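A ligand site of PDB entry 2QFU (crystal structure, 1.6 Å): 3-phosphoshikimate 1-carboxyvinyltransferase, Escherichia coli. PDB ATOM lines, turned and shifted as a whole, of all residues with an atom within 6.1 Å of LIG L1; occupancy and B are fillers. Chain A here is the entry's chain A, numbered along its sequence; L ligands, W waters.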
ATOM      1  N   LYS A  22      11.652 -21.768  27.764  1.00  0.00           N
ATOM      2  CA  LYS A  22      10.668 -21.890  26.685  1.00  0.00           C
ATOM      3  C   LYS A  22      10.128 -20.499  26.313  1.00  0.00           C
ATOM      4  O   LYS A  22      10.000 -20.160  25.139  1.00  0.00           O
ATOM      5  CB  LYS A  22       9.495 -22.785  27.154  1.00  0.00           C
ATOM      6  CG  LYS A  22       8.323 -22.846  26.159  1.00  0.00           C
ATOM      7  CD  LYS A  22       7.035 -22.232  26.723  1.00  0.00           C
ATOM      8  CE  LYS A  22       6.404 -23.177  27.745  1.00  0.00           C
ATOM      9  NZ  LYS A  22       5.332 -22.476  28.506  1.00  0.00           N
ATOM     10  N   ASP A  49       7.274 -27.389  22.434  1.00  0.00           N
ATOM     11  CA  ASP A  49       6.792 -26.036  22.150  1.00  0.00           C
ATOM     12  C   ASP A  49       7.719 -25.243  21.253  1.00  0.00           C
ATOM     13  O   ASP A  49       7.246 -24.457  20.442  1.00  0.00           O
ATOM     14  CB  ASP A  49       6.548 -25.250  23.448  1.00  0.00           C
ATOM     15  CG  ASP A  49       5.283 -25.669  24.159  1.00  0.00           C
ATOM     16  OD1 ASP A  49       4.564 -26.576  23.678  1.00  0.00           O
ATOM     17  OD2 ASP A  49       5.020 -25.065  25.206  1.00  0.00           O
ATOM     18  N   ASN A  94       0.363 -27.877  21.469  1.00  0.00           N
ATOM     19  CA  ASN A  94      -0.395 -27.225  22.532  1.00  0.00           C
ATOM     20  C   ASN A  94       0.471 -26.088  23.063  1.00  0.00           C
ATOM     21  O   ASN A  94       0.426 -25.742  24.248  1.00  0.00           O
ATOM     22  CB  ASN A  94      -0.764 -28.172  23.678  1.00  0.00           C
ATOM     23  CG  ASN A  94      -1.863 -27.606  24.570  1.00  0.00           C
ATOM     24  OD1 ASN A  94      -2.540 -26.639  24.210  1.00  0.00           O
ATOM     25  ND2 ASN A  94      -2.062 -28.226  25.735  1.00  0.00           N
ATOM     26  N   ALA A  95       1.236 -25.496  22.144  1.00  0.00           N
ATOM     27  CA  ALA A  95       2.135 -24.386  22.505  1.00  0.00           C
ATOM     28  C   ALA A  95       1.425 -23.039  22.477  1.00  0.00           C
ATOM     29  O   ALA A  95       1.310 -22.413  21.424  1.00  0.00           O
ATOM     30  CB  ALA A  95       3.341 -24.365  21.547  1.00  0.00           C
ATOM     31  N   GLY A  96       0.982 -22.580  23.642  1.00  0.00           N
ATOM     32  CA  GLY A  96       0.311 -21.296  23.678  1.00  0.00           C
ATOM     33  C   GLY A  96       1.238 -20.174  23.217  1.00  0.00           C
ATOM     34  O   GLY A  96       0.806 -19.240  22.524  1.00  0.00           O
ATOM     35  N   THR A  97       2.508 -20.249  23.581  1.00  0.00           N
ATOM     36  CA  THR A  97       3.397 -19.163  23.179  1.00  0.00           C
ATOM     37  C   THR A  97       3.492 -19.089  21.674  1.00  0.00           C
ATOM     38  O   THR A  97       3.630 -17.999  21.122  1.00  0.00           O
ATOM     39  CB  THR A  97       4.807 -19.282  23.812  1.00  0.00           C
ATOM     40  OG1 THR A  97       5.389 -20.572  23.548  1.00  0.00           O
ATOM     41  CG2 THR A  97       4.719 -19.080  25.312  1.00  0.00           C
ATOM     42  N   ARG A 100      -0.502 -17.974  20.411  1.00  0.00           N
ATOM     43  CA  ARG A 100      -0.875 -16.586  20.652  1.00  0.00           C
ATOM     44  C   ARG A 100       0.037 -15.612  19.917  1.00  0.00           C
ATOM     45  O   ARG A 100      -0.448 -14.673  19.280  1.00  0.00           O
ATOM     46  CB  ARG A 100      -0.865 -16.286  22.162  1.00  0.00           C
ATOM     47  CG  ARG A 100      -2.146 -16.700  22.904  1.00  0.00           C
ATOM     48  CD  ARG A 100      -2.317 -18.232  22.900  1.00  0.00           C
ATOM     49  NE  ARG A 100      -3.464 -18.666  23.707  1.00  0.00           N
ATOM     50  CZ  ARG A 100      -3.443 -18.956  25.009  1.00  0.00           C
ATOM     51  NH1 ARG A 100      -4.568 -19.349  25.619  1.00  0.00           N
ATOM     52  NH2 ARG A 100      -2.322 -18.865  25.718  1.00  0.00           N
ATOM     53  N   MET A 121      -5.630 -27.716  22.513  1.00  0.00           N
ATOM     54  CA  MET A 121      -5.442 -26.324  22.120  1.00  0.00           C
ATOM     55  C   MET A 121      -6.730 -25.698  21.578  1.00  0.00           C
ATOM     56  O   MET A 121      -6.925 -24.473  21.680  1.00  0.00           O
ATOM     57  CB  MET A 121      -4.312 -26.215  21.076  1.00  0.00           C
ATOM     58  CG  MET A 121      -4.084 -24.814  20.512  1.00  0.00           C
ATOM     59  SD  MET A 121      -3.745 -23.514  21.748  1.00  0.00           S
ATOM     60  CE  MET A 121      -2.008 -23.894  22.171  1.00  0.00           C
ATOM     61  N   ARG A 124      -8.449 -24.025  24.438  1.00  0.00           N
ATOM     62  CA  ARG A 124      -7.760 -22.968  25.189  1.00  0.00           C
ATOM     63  C   ARG A 124      -8.144 -21.651  24.549  1.00  0.00           C
ATOM     64  O   ARG A 124      -7.983 -21.461  23.343  1.00  0.00           O
ATOM     65  CB  ARG A 124      -6.257 -23.225  25.170  1.00  0.00           C
ATOM     66  CG  ARG A 124      -5.913 -24.474  26.010  1.00  0.00           C
ATOM     67  CD  ARG A 124      -4.418 -24.688  26.111  1.00  0.00           C
ATOM     68  NE  ARG A 124      -3.799 -23.555  26.782  1.00  0.00           N
ATOM     69  CZ  ARG A 124      -2.502 -23.255  26.717  1.00  0.00           C
ATOM     70  NH1 ARG A 124      -2.046 -22.193  27.379  1.00  0.00           N
ATOM     71  NH2 ARG A 124      -1.671 -24.008  26.008  1.00  0.00           N
ATOM     72  N   GLN A 171      -0.491 -13.557  27.595  1.00  0.00           N
ATOM     73  CA  GLN A 171       0.031 -13.781  26.258  1.00  0.00           C
ATOM     74  C   GLN A 171      -0.643 -12.965  25.174  1.00  0.00           C
ATOM     75  O   GLN A 171      -0.046 -12.693  24.124  1.00  0.00           O
ATOM     76  CB  GLN A 171      -0.056 -15.259  25.890  1.00  0.00           C
ATOM     77  CG  GLN A 171       0.924 -16.118  26.693  1.00  0.00           C
ATOM     78  CD  GLN A 171       0.866 -17.563  26.270  1.00  0.00           C
ATOM     79  OE1 GLN A 171       0.290 -17.899  25.238  1.00  0.00           O
ATOM     80  NE2 GLN A 171       1.507 -18.440  27.050  1.00  0.00           N
ATOM     81  N   ASP A 313       3.095 -20.978  36.881  1.00  0.00           N
ATOM     82  CA  ASP A 313       3.648 -22.270  36.457  1.00  0.00           C
ATOM     83  C   ASP A 313       4.462 -22.908  37.574  1.00  0.00           C
ATOM     84  O   ASP A 313       4.212 -24.037  37.975  1.00  0.00           O
ATOM     85  CB  ASP A 313       4.517 -22.099  35.209  1.00  0.00           C
ATOM     86  CG  ASP A 313       3.716 -21.650  33.996  1.00  0.00           C
ATOM     87  OD1 ASP A 313       4.362 -21.422  32.945  1.00  0.00           O
ATOM     88  OD2 ASP A 313       2.478 -21.535  34.076  1.00  0.00           O
ATOM     89  N   MET A 316       2.798 -24.577  40.682  1.00  0.00           N
ATOM     90  CA  MET A 316       2.332 -25.963  40.766  1.00  0.00           C
ATOM     91  C   MET A 316       3.317 -26.795  41.588  1.00  0.00           C
ATOM     92  O   MET A 316       2.923 -27.758  42.262  1.00  0.00           O
ATOM     93  CB  MET A 316       2.200 -26.564  39.375  1.00  0.00           C
ATOM     94  CG  MET A 316       1.225 -25.856  38.459  1.00  0.00           C
ATOM     95  SD  MET A 316       1.188 -26.639  36.830  1.00  0.00           S
ATOM     96  CE  MET A 316       0.583 -28.341  37.204  1.00  0.00           C
ATOM     97  N   LYS A 340      -5.010 -23.940  30.905  1.00  0.00           N
ATOM     98  CA  LYS A 340      -3.696 -24.228  30.359  1.00  0.00           C
ATOM     99  C   LYS A 340      -3.601 -25.649  29.794  1.00  0.00           C
ATOM    100  O   LYS A 340      -4.587 -26.105  29.217  1.00  0.00           O
ATOM    101  CB  LYS A 340      -2.627 -23.879  31.408  1.00  0.00           C
ATOM    102  CG  LYS A 340      -2.417 -22.342  31.398  1.00  0.00           C
ATOM    103  CD  LYS A 340      -1.579 -21.824  32.519  1.00  0.00           C
ATOM    104  CE  LYS A 340      -1.358 -20.319  32.289  1.00  0.00           C
ATOM    105  NZ  LYS A 340      -0.724 -19.703  33.479  1.00  0.00           N
ATOM    106  N   GLU A 341      -2.471 -26.352  29.950  1.00  0.00           N
ATOM    107  CA  GLU A 341      -2.356 -27.686  29.330  1.00  0.00           C
ATOM    108  C   GLU A 341      -3.488 -28.623  29.643  1.00  0.00           C
ATOM    109  O   GLU A 341      -3.845 -29.472  28.816  1.00  0.00           O
ATOM    110  CB  GLU A 341      -1.015 -28.323  29.677  1.00  0.00           C
ATOM    111  CG  GLU A 341       0.177 -27.704  28.885  1.00  0.00           C
ATOM    112  CD  GLU A 341       0.739 -26.375  29.445  1.00  0.00           C
ATOM    113  OE1 GLU A 341       0.027 -25.654  30.187  1.00  0.00           O
ATOM    114  OE2 GLU A 341       1.893 -26.053  29.104  1.00  0.00           O
ATOM    115  N   ARG A 344      -5.668 -27.411  35.457  1.00  0.00           N
ATOM    116  CA  ARG A 344      -4.736 -27.787  36.511  1.00  0.00           C
ATOM    117  C   ARG A 344      -5.269 -27.746  37.922  1.00  0.00           C
ATOM    118  O   ARG A 344      -4.753 -28.427  38.799  1.00  0.00           O
ATOM    119  CB  ARG A 344      -3.479 -26.941  36.388  1.00  0.00           C
ATOM    120  CG  ARG A 344      -2.700 -27.299  35.141  1.00  0.00           C
ATOM    121  CD  ARG A 344      -1.668 -26.211  34.786  1.00  0.00           C
ATOM    122  NE  ARG A 344      -0.574 -26.799  34.012  1.00  0.00           N
ATOM    123  CZ  ARG A 344       0.490 -26.126  33.573  1.00  0.00           C
ATOM    124  NH1 ARG A 344       1.427 -26.762  32.888  1.00  0.00           N
ATOM    125  NH2 ARG A 344       0.598 -24.816  33.826  1.00  0.00           N
ATOM    126  N   ASP A 384       0.096 -33.096  30.421  1.00  0.00           N
ATOM    127  CA  ASP A 384       0.654 -31.883  31.009  1.00  0.00           C
ATOM    128  C   ASP A 384       2.012 -32.136  31.636  1.00  0.00           C
ATOM    129  O   ASP A 384       2.113 -32.709  32.714  1.00  0.00           O
ATOM    130  CB  ASP A 384      -0.340 -31.349  32.052  1.00  0.00           C
ATOM    131  CG  ASP A 384       0.110 -30.050  32.690  1.00  0.00           C
ATOM    132  OD1 ASP A 384       1.245 -29.604  32.412  1.00  0.00           O
ATOM    133  OD2 ASP A 384      -0.672 -29.492  33.479  1.00  0.00           O
ATOM    134  N   HIS A 385       3.055 -31.681  30.922  1.00  0.00           N
ATOM    135  CA  HIS A 385       4.433 -31.812  31.416  1.00  0.00           C
ATOM    136  C   HIS A 385       4.583 -31.521  32.902  1.00  0.00           C
ATOM    137  O   HIS A 385       5.284 -32.258  33.608  1.00  0.00           O
ATOM    138  CB  HIS A 385       5.373 -30.862  30.627  1.00  0.00           C
ATOM    139  CG  HIS A 385       4.935 -29.437  30.579  1.00  0.00           C
ATOM    140  ND1 HIS A 385       5.817 -28.389  30.697  1.00  0.00           N
ATOM    141  CD2 HIS A 385       3.707 -28.872  30.400  1.00  0.00           C
ATOM    142  CE1 HIS A 385       5.172 -27.239  30.596  1.00  0.00           C
ATOM    143  NE2 HIS A 385       3.888 -27.503  30.420  1.00  0.00           N
ATOM    144  N   ARG A 386       3.925 -30.467  33.393  1.00  0.00           N
ATOM    145  CA  ARG A 386       4.096 -30.137  34.805  1.00  0.00           C
ATOM    146  C   ARG A 386       3.430 -31.073  35.787  1.00  0.00           C
ATOM    147  O   ARG A 386       3.844 -31.163  36.942  1.00  0.00           O
ATOM    148  CB  ARG A 386       3.699 -28.672  35.061  1.00  0.00           C
ATOM    149  CG  ARG A 386       4.599 -27.700  34.274  1.00  0.00           C
ATOM    150  CD  ARG A 386       4.687 -26.279  34.914  1.00  0.00           C
ATOM    151  NE  ARG A 386       5.244 -25.405  33.884  1.00  0.00           N
ATOM    152  CZ  ARG A 386       6.509 -25.406  33.473  1.00  0.00           C
ATOM    153  NH1 ARG A 386       6.844 -24.606  32.457  1.00  0.00           N
ATOM    154  NH2 ARG A 386       7.463 -26.103  34.107  1.00  0.00           N
ATOM    155  N   LYS A 411       7.091 -31.371  26.516  1.00  0.00           N
ATOM    156  CA  LYS A 411       6.561 -30.083  26.079  1.00  0.00           C
ATOM    157  C   LYS A 411       7.586 -28.977  26.368  1.00  0.00           C
ATOM    158  O   LYS A 411       7.750 -28.057  25.540  1.00  0.00           O
ATOM    159  CB  LYS A 411       5.239 -29.750  26.792  1.00  0.00           C
ATOM    160  CG  LYS A 411       4.488 -28.581  26.126  1.00  0.00           C
ATOM    161  CD  LYS A 411       3.072 -28.426  26.686  1.00  0.00           C
ATOM    162  CE  LYS A 411       2.283 -27.391  25.896  1.00  0.00           C
ATOM    163  NZ  LYS A 411       2.644 -26.007  26.349  1.00  0.00           N
ATOM    164  N   THR A 412       8.293 -29.081  27.494  1.00  0.00           N
ATOM    165  CA  THR A 412       9.298 -28.099  27.869  1.00  0.00           C
ATOM    166  C   THR A 412      10.588 -28.677  28.405  1.00  0.00           C
ATOM    167  O   THR A 412      11.547 -27.957  28.567  1.00  0.00           O
ATOM    168  CB  THR A 412       8.804 -27.158  29.014  1.00  0.00           C
ATOM    169  OG1 THR A 412       8.495 -27.954  30.181  1.00  0.00           O
ATOM    170  CG2 THR A 412       7.575 -26.358  28.569  1.00  0.00           C
HETATM  171  P1  LIG L   1       1.422 -22.252  27.191  1.00  0.00           P
HETATM  172  O1  LIG L   1       2.867 -21.931  27.134  1.00  0.00           O
HETATM  173  O2  LIG L   1       0.522 -21.124  26.875  1.00  0.00           O
HETATM  174  O3  LIG L   1       1.120 -23.474  26.344  1.00  0.00           O
HETATM  175  O4  LIG L   1       4.273 -24.052  30.811  1.00  0.00           O
HETATM  176  O5  LIG L   1       3.185 -24.405  32.701  1.00  0.00           O
HETATM  177  C1  LIG L   1       1.018 -22.620  28.822  1.00  0.00           C
HETATM  178  C2  LIG L   1       1.966 -23.514  30.961  1.00  0.00           C
HETATM  179  C3  LIG L   1       3.233 -24.028  31.540  1.00  0.00           C
HETATM  180  N1  LIG L   1       2.143 -23.149  29.553  1.00  0.00           N
HETATM  181  C1  LG2 L   2       4.022 -17.491  29.229  1.00  0.00           C
HETATM  182  C2  LG2 L   2       3.000 -16.900  29.987  1.00  0.00           C
HETATM  183  C3  LG2 L   2       2.147 -17.716  30.926  1.00  0.00           C
HETATM  184  C4  LG2 L   2       2.758 -19.091  31.254  1.00  0.00           C
HETATM  185  C5  LG2 L   2       3.280 -19.777  29.987  1.00  0.00           C
HETATM  186  C6  LG2 L   2       4.345 -18.886  29.344  1.00  0.00           C
HETATM  187  C7  LG2 L   2       4.813 -16.631  28.284  1.00  0.00           C
HETATM  188  O1  LG2 L   2       0.773 -17.776  30.430  1.00  0.00           O
HETATM  189  O2  LG2 L   2       1.783 -19.879  31.968  1.00  0.00           O
HETATM  190  O3  LG2 L   2       3.851 -21.053  30.299  1.00  0.00           O
HETATM  191  O4  LG2 L   2       4.310 -15.542  27.924  1.00  0.00           O
HETATM  192  O5  LG2 L   2       5.934 -17.014  27.960  1.00  0.00           O
HETATM  193  P1  LG2 L   2      -0.510 -16.859  30.977  1.00  0.00           P
HETATM  194  O6  LG2 L   2      -0.146 -15.445  30.704  1.00  0.00           O
HETATM  195  O7  LG2 L   2      -0.603 -17.167  32.452  1.00  0.00           O
HETATM  196  O8  LG2 L   2      -1.686 -17.307  30.182  1.00  0.00           O
HETATM  197  O   HOH W   1      -1.364 -19.515  28.508  1.00  0.00           O
HETATM  198  O   HOH W   2       4.110 -22.443  24.903  1.00  0.00           O
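The backbone carbonyl oxygen of Asn 94 lies within hydrogen-bond range of the guanidinium group of Arg 124 (3.2 Å).
The backbone carbonyl oxygen (O) of Gly 96 lies close to the side-chain amide oxygen (OE1) of Gln 171.
NH1 of Arg 344 is in salt-bridge range of OE1 of Glu 341, 3.2 Å away.
The guanidinium group (NH2) of Arg 344 is in salt-bridge range of the side-chain carboxylate (OD2) of Asp 313.
The guanidinium group (NE) of Arg 344 is in salt-bridge range of the side-chain carboxylate (OD2) of Asp 384 (2.7 Å).
NZ of Lys 411 is in salt-bridge range of OE2 of Glu 341, 2.9 Å away.
NZ of Lys 411 lies within salt-bridge range of OD2 of Asp 49 (2.8 Å).
The side-chain amino group (NZ) of Lys 340 is in salt-bridge range of the side-chain carboxylate (OD2) of Asp 313, 3.7 Å away.
Water W2 lies within hydrogen-bond range of an oxygen (O1) of LIG L1, the side-chain hydroxyl (OG1) of Thr 97, the side-chain carboxylate (OD2) of Asp 49 and the backbone NH (N) of Gly 96.
The guanidinium group (NE) of Arg 386 is in salt-bridge range of an oxygen (O5) of LIG L1, at 2.6 Å.
The guanidinium group of Arg 124 lies within salt-bridge range of an oxygen (O2) of LIG L1 (2.8 Å).
The backbone NH (N) of Gly 96 lies within hydrogen-bond range of an oxygen (O3) of LIG L1, at 2.8 Å.
The guanidinium group of Arg 344 is in salt-bridge range of an oxygen (O5) of LIG L1 (2.9 Å).
The side-chain amide nitrogen (NE2) of Gln 171 is in hydrogen-bond range of an oxygen (O2) of LIG L1, 2.9 Å away.
The side-chain amino group (NZ) of Lys 22 is in salt-bridge range of an oxygen (O1) of LIG L1 (2.9 Å).
N1 of LIG L1 lies within salt-bridge range of OE2 of Glu 341.
NZ of Lys 411 lies within salt-bridge range of O3 of LIG L1 (3.0 Å).
A ring nitrogen (NE2) of His 385 lies close to an oxygen (O4) of LIG L1, 3.5 Å away.
The guanidinium group (NH2) of Arg 100 is in salt-bridge range of an oxygen (O2) of LIG L1, 3.8 Å away.
The side-chain amino group (NZ) of Lys 22 is in hydrogen-bond range of an oxygen (O3) of LG2 L2 (2.7 Å).
The side-chain carboxylate (OD1) of Asp 313 lies within hydrogen-bond range of an oxygen (O3) of LG2 L2, 2.7 Å away.
The side-chain amino group (NZ) of Lys 340 is in salt-bridge range of an oxygen (O7) of LG2 L2, at 2.7 Å.
O of Asn 94 lies close to O3 of LIG L1, at 3.2 Å.
OD1 of Asp 313 sits close to O5 of LIG L1, at 3.2 Å.
C of Ala 95 touches O3 of LIG L1, at 3.9 Å.
Thr 97 touches LIG L1 (CG2 to O1, 3.9 Å).
Hydrophobic or aromatic side chains within 4 Å of LIG L1: His 385.
Of the 20 residues printed, 14 come within 4 Å of LIG L1.
The nearest printed residue that does not touch LIG L1 is Lys 340 (4.2 Å).
N1 of LIG L1 lies within hydrogen-bond range of O3 of LG2 L2, 2.8 Å away.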
